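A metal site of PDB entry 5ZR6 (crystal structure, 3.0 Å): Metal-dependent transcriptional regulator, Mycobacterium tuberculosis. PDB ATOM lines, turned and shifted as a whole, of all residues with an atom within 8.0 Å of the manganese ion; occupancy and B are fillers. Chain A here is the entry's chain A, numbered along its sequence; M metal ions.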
ATOM      1  N   VAL A   3      26.035  -6.031   6.225  1.00  0.00           N
ATOM      2  CA  VAL A   3      26.665  -7.344   6.284  1.00  0.00           C
ATOM      3  C   VAL A   3      26.404  -8.106   4.985  1.00  0.00           C
ATOM      4  O   VAL A   3      25.269  -8.475   4.685  1.00  0.00           O
ATOM      5  CB  VAL A   3      26.174  -8.124   7.502  1.00  0.00           C
ATOM      6  CG1 VAL A   3      26.974  -7.721   8.731  1.00  0.00           C
ATOM      7  CG2 VAL A   3      24.703  -7.851   7.751  1.00  0.00           C
ATOM      8  N   GLN A   5      27.042 -11.096   3.882  1.00  0.00           N
ATOM      9  CA  GLN A   5      26.496 -12.452   3.926  1.00  0.00           C
ATOM     10  C   GLN A   5      24.996 -12.460   4.137  1.00  0.00           C
ATOM     11  O   GLN A   5      24.306 -13.386   3.686  1.00  0.00           O
ATOM     12  CB  GLN A   5      27.183 -13.261   5.036  1.00  0.00           C
ATOM     13  CG  GLN A   5      28.707 -13.177   5.021  1.00  0.00           C
ATOM     14  CD  GLN A   5      29.326 -13.814   6.249  1.00  0.00           C
ATOM     15  OE1 GLN A   5      29.744 -14.970   6.226  1.00  0.00           O
ATOM     16  NE2 GLN A   5      29.384 -13.052   7.344  1.00  0.00           N
ATOM     17  N   ASP A   6      24.466 -11.442   4.830  1.00  0.00           N
ATOM     18  CA  ASP A   6      23.021 -11.368   5.051  1.00  0.00           C
ATOM     19  C   ASP A   6      22.252 -11.279   3.742  1.00  0.00           C
ATOM     20  O   ASP A   6      21.149 -11.815   3.636  1.00  0.00           O
ATOM     21  CB  ASP A   6      22.694 -10.182   5.949  1.00  0.00           C
ATOM     22  CG  ASP A   6      22.507 -10.567   7.394  1.00  0.00           C
ATOM     23  OD1 ASP A   6      22.754 -11.748   7.731  1.00  0.00           O
ATOM     24  OD2 ASP A   6      22.130  -9.694   8.210  1.00  0.00           O
ATOM     25  N   TYR A   7      22.818 -10.598   2.750  1.00  0.00           N
ATOM     26  CA  TYR A   7      22.119 -10.396   1.483  1.00  0.00           C
ATOM     27  C   TYR A   7      21.909 -11.711   0.742  1.00  0.00           C
ATOM     28  O   TYR A   7      20.792 -12.004   0.299  1.00  0.00           O
ATOM     29  CB  TYR A   7      22.873  -9.389   0.618  1.00  0.00           C
ATOM     30  CG  TYR A   7      22.726  -7.959   1.105  1.00  0.00           C
ATOM     31  CD1 TYR A   7      23.484  -7.487   2.172  1.00  0.00           C
ATOM     32  CD2 TYR A   7      21.818  -7.096   0.514  1.00  0.00           C
ATOM     33  CE1 TYR A   7      23.345  -6.189   2.630  1.00  0.00           C
ATOM     34  CE2 TYR A   7      21.674  -5.798   0.959  1.00  0.00           C
ATOM     35  CZ  TYR A   7      22.442  -5.351   2.014  1.00  0.00           C
ATOM     36  OH  TYR A   7      22.306  -4.056   2.462  1.00  0.00           O
ATOM     37  N   LYS A   9      21.839 -14.791   1.840  1.00  0.00           N
ATOM     38  CA  LYS A   9      20.886 -15.625   2.548  1.00  0.00           C
ATOM     39  C   LYS A   9      19.462 -15.097   2.369  1.00  0.00           C
ATOM     40  O   LYS A   9      18.525 -15.874   2.196  1.00  0.00           O
ATOM     41  CB  LYS A   9      21.237 -15.704   4.032  1.00  0.00           C
ATOM     42  CG  LYS A   9      20.400 -16.715   4.802  1.00  0.00           C
ATOM     43  CD  LYS A   9      20.468 -16.519   6.304  1.00  0.00           C
ATOM     44  CE  LYS A   9      20.001 -15.125   6.697  1.00  0.00           C
ATOM     45  NZ  LYS A   9      20.043 -14.936   8.180  1.00  0.00           N
ATOM     46  N   VAL A  10      19.302 -13.777   2.399  1.00  0.00           N
ATOM     47  CA  VAL A  10      17.971 -13.193   2.262  1.00  0.00           C
ATOM     48  C   VAL A  10      17.442 -13.382   0.846  1.00  0.00           C
ATOM     49  O   VAL A  10      16.268 -13.724   0.656  1.00  0.00           O
ATOM     50  CB  VAL A  10      17.994 -11.713   2.677  1.00  0.00           C
ATOM     51  CG1 VAL A  10      16.780 -10.995   2.123  1.00  0.00           C
ATOM     52  CG2 VAL A  10      18.033 -11.581   4.194  1.00  0.00           C
ATOM     53  N   ILE A  31      16.315  -6.821   5.544  1.00  0.00           N
ATOM     54  CA  ILE A  31      17.636  -6.902   6.141  1.00  0.00           C
ATOM     55  C   ILE A  31      17.759  -5.918   7.292  1.00  0.00           C
ATOM     56  O   ILE A  31      18.478  -6.160   8.272  1.00  0.00           O
ATOM     57  CB  ILE A  31      18.720  -6.683   5.055  1.00  0.00           C
ATOM     58  CG1 ILE A  31      18.802  -7.912   4.147  1.00  0.00           C
ATOM     59  CG2 ILE A  31      20.075  -6.372   5.677  1.00  0.00           C
ATOM     60  CD1 ILE A  31      20.092  -8.029   3.391  1.00  0.00           C
ATOM     61  N   MET A  72      25.158 -20.108   4.128  1.00  0.00           N
ATOM     62  CA  MET A  72      24.610 -19.250   5.170  1.00  0.00           C
ATOM     63  C   MET A  72      23.298 -19.798   5.712  1.00  0.00           C
ATOM     64  O   MET A  72      23.064 -19.788   6.923  1.00  0.00           O
ATOM     65  CB  MET A  72      24.397 -17.828   4.623  1.00  0.00           C
ATOM     66  CG  MET A  72      25.651 -16.961   4.624  1.00  0.00           C
ATOM     67  SD  MET A  72      26.343 -16.666   6.257  1.00  0.00           S
ATOM     68  CE  MET A  72      27.842 -17.642   6.169  1.00  0.00           C
ATOM     69  N   HIS A  76      22.556 -20.823   9.691  1.00  0.00           N
ATOM     70  CA  HIS A  76      21.422 -20.214  10.380  1.00  0.00           C
ATOM     71  C   HIS A  76      20.448 -21.271  10.896  1.00  0.00           C
ATOM     72  O   HIS A  76      19.991 -21.205  12.035  1.00  0.00           O
ATOM     73  CB  HIS A  76      20.699 -19.244   9.436  1.00  0.00           C
ATOM     74  CG  HIS A  76      19.449 -18.652  10.023  1.00  0.00           C
ATOM     75  ND1 HIS A  76      19.438 -17.448  10.690  1.00  0.00           N
ATOM     76  CD2 HIS A  76      18.176 -19.095  10.030  1.00  0.00           C
ATOM     77  CE1 HIS A  76      18.215 -17.176  11.082  1.00  0.00           C
ATOM     78  NE2 HIS A  76      17.422 -18.159  10.696  1.00  0.00           N
ATOM     79  N   HIS A  95      15.339 -17.134  16.088  1.00  0.00           N
ATOM     80  CA  HIS A  95      15.720 -16.500  14.824  1.00  0.00           C
ATOM     81  C   HIS A  95      16.619 -15.298  15.052  1.00  0.00           C
ATOM     82  O   HIS A  95      17.601 -15.102  14.317  1.00  0.00           O
ATOM     83  CB  HIS A  95      14.482 -16.105  14.036  1.00  0.00           C
ATOM     84  CG  HIS A  95      14.794 -15.640  12.648  1.00  0.00           C
ATOM     85  ND1 HIS A  95      15.023 -16.509  11.604  1.00  0.00           N
ATOM     86  CD2 HIS A  95      14.941 -14.390  12.129  1.00  0.00           C
ATOM     87  CE1 HIS A  95      15.284 -15.819  10.502  1.00  0.00           C
ATOM     88  NE2 HIS A  95      15.248 -14.541  10.804  1.00  0.00           N
ATOM     89  N   ASP A  96      16.306 -14.467  16.043  1.00  0.00           N
ATOM     90  CA  ASP A  96      17.150 -13.307  16.306  1.00  0.00           C
ATOM     91  C   ASP A  96      18.537 -13.713  16.800  1.00  0.00           C
ATOM     92  O   ASP A  96      19.522 -13.004  16.549  1.00  0.00           O
ATOM     93  CB  ASP A  96      16.474 -12.379  17.318  1.00  0.00           C
ATOM     94  CG  ASP A  96      15.105 -11.912  16.836  1.00  0.00           C
ATOM     95  OD1 ASP A  96      14.895 -11.860  15.615  1.00  0.00           O
ATOM     96  OD2 ASP A  96      14.261 -11.590  17.699  1.00  0.00           O
ATOM     97  N   GLU A  97      18.630 -14.864  17.478  1.00  0.00           N
ATOM     98  CA  GLU A  97      19.932 -15.323  17.967  1.00  0.00           C
ATOM     99  C   GLU A  97      20.785 -15.848  16.820  1.00  0.00           C
ATOM    100  O   GLU A  97      21.927 -15.401  16.624  1.00  0.00           O
ATOM    101  CB  GLU A  97      19.733 -16.402  19.024  1.00  0.00           C
ATOM    102  CG  GLU A  97      21.011 -16.798  19.739  1.00  0.00           C
ATOM    103  CD  GLU A  97      21.450 -15.772  20.752  1.00  0.00           C
ATOM    104  OE1 GLU A  97      22.564 -15.217  20.596  1.00  0.00           O
ATOM    105  OE2 GLU A  97      20.687 -15.508  21.713  1.00  0.00           O
ATOM    106  N   ALA A  98      20.264 -16.806  16.044  1.00  0.00           N
ATOM    107  CA  ALA A  98      21.019 -17.362  14.935  1.00  0.00           C
ATOM    108  C   ALA A  98      21.259 -16.355  13.823  1.00  0.00           C
ATOM    109  O   ALA A  98      22.136 -16.565  12.987  1.00  0.00           O
ATOM    110  CB  ALA A  98      20.294 -18.589  14.372  1.00  0.00           C
ATOM    111  N   GLU A  99      20.509 -15.244  13.804  1.00  0.00           N
ATOM    112  CA  GLU A  99      20.769 -14.201  12.821  1.00  0.00           C
ATOM    113  C   GLU A  99      22.089 -13.485  13.101  1.00  0.00           C
ATOM    114  O   GLU A  99      22.715 -12.954  12.189  1.00  0.00           O
ATOM    115  CB  GLU A  99      19.612 -13.204  12.806  1.00  0.00           C
ATOM    116  CG  GLU A  99      19.725 -12.102  11.756  1.00  0.00           C
ATOM    117  CD  GLU A  99      19.611 -12.628  10.342  1.00  0.00           C
ATOM    118  OE1 GLU A  99      18.721 -13.462  10.080  1.00  0.00           O
ATOM    119  OE2 GLU A  99      20.411 -12.205   9.486  1.00  0.00           O
ATOM    120  N   VAL A 100      22.522 -13.483  14.366  1.00  0.00           N
ATOM    121  CA  VAL A 100      23.800 -12.887  14.748  1.00  0.00           C
ATOM    122  C   VAL A 100      24.905 -13.924  14.819  1.00  0.00           C
ATOM    123  O   VAL A 100      26.044 -13.651  14.437  1.00  0.00           O
ATOM    124  CB  VAL A 100      23.650 -12.127  16.086  1.00  0.00           C
ATOM    125  CG1 VAL A 100      24.901 -11.328  16.387  1.00  0.00           C
ATOM    126  CG2 VAL A 100      22.425 -11.232  16.051  1.00  0.00           C
ATOM    127  N   LEU A 101      24.589 -15.122  15.320  1.00  0.00           N
ATOM    128  CA  LEU A 101      25.575 -16.192  15.455  1.00  0.00           C
ATOM    129  C   LEU A 101      26.036 -16.749  14.123  1.00  0.00           C
ATOM    130  O   LEU A 101      27.034 -17.481  14.092  1.00  0.00           O
ATOM    131  CB  LEU A 101      24.997 -17.318  16.314  1.00  0.00           C
ATOM    132  CG  LEU A 101      25.569 -17.498  17.717  1.00  0.00           C
ATOM    133  CD1 LEU A 101      25.202 -18.864  18.263  1.00  0.00           C
ATOM    134  CD2 LEU A 101      27.084 -17.320  17.687  1.00  0.00           C
ATOM    135  N   GLU A 102      25.360 -16.432  13.020  1.00  0.00           N
ATOM    136  CA  GLU A 102      25.670 -17.047  11.735  1.00  0.00           C
ATOM    137  C   GLU A 102      26.989 -16.561  11.145  1.00  0.00           C
ATOM    138  O   GLU A 102      27.581 -17.279  10.335  1.00  0.00           O
ATOM    139  CB  GLU A 102      24.529 -16.781  10.752  1.00  0.00           C
ATOM    140  CG  GLU A 102      24.222 -15.313  10.541  1.00  0.00           C
ATOM    141  CD  GLU A 102      22.939 -15.078   9.788  1.00  0.00           C
ATOM    142  OE1 GLU A 102      22.660 -13.916   9.412  1.00  0.00           O
ATOM    143  OE2 GLU A 102      22.174 -16.051   9.583  1.00  0.00           O
ATOM    144  N   HIS A 103      27.465 -15.372  11.521  1.00  0.00           N
ATOM    145  CA  HIS A 103      28.680 -14.814  10.953  1.00  0.00           C
ATOM    146  C   HIS A 103      29.913 -15.041  11.806  1.00  0.00           C
ATOM    147  O   HIS A 103      30.985 -14.514  11.468  1.00  0.00           O
ATOM    148  CB  HIS A 103      28.513 -13.308  10.684  1.00  0.00           C
ATOM    149  CG  HIS A 103      27.141 -12.917  10.253  1.00  0.00           C
ATOM    150  ND1 HIS A 103      26.740 -12.936   8.928  1.00  0.00           N
ATOM    151  CD2 HIS A 103      26.082 -12.449  10.959  1.00  0.00           C
ATOM    152  CE1 HIS A 103      25.497 -12.524   8.842  1.00  0.00           C
ATOM    153  NE2 HIS A 103      25.067 -12.223  10.053  1.00  0.00           N
HETATM  154 MN    MN M   1      22.679 -12.126  10.206  1.00  0.00          MN
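The manganese ion is bound by OE1 of Glu 102.
The backbone carbonyl oxygen (O) of Glu 99 is bound to the manganese ion (2.1 Å).
The manganese ion is bound by OE2 of Glu 99, 2.4 Å away.
The manganese ion is bound by NE2 of His 103 (2.4 Å).
The manganese ion is bound by OD1 of Asp 6 (2.5 Å).
The manganese ion has five donor atoms within binding distance.
Within 4 Å of the manganese ion: Asp 6, Glu 99, Glu 102 and His 103.
Along chain A the residues within 4 Å of the manganese ion span positions 6 to 103.
The side-chain carboxylate of Glu 102 is in salt-bridge range of the side-chain amino group of Lys 9 (2.8 Å).
OE2 of Glu 102 lies within hydrogen-bond range of ND1 of His 76 (3.3 Å).
The side-chain carboxylate (OE1) of Glu 99 lies within salt-bridge range of the side-chain amino group (NZ) of Lys 9 (2.7 Å).
ND1 of His 103 is in hydrogen-bond range of NE2 of Gln 5 (3.1 Å).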
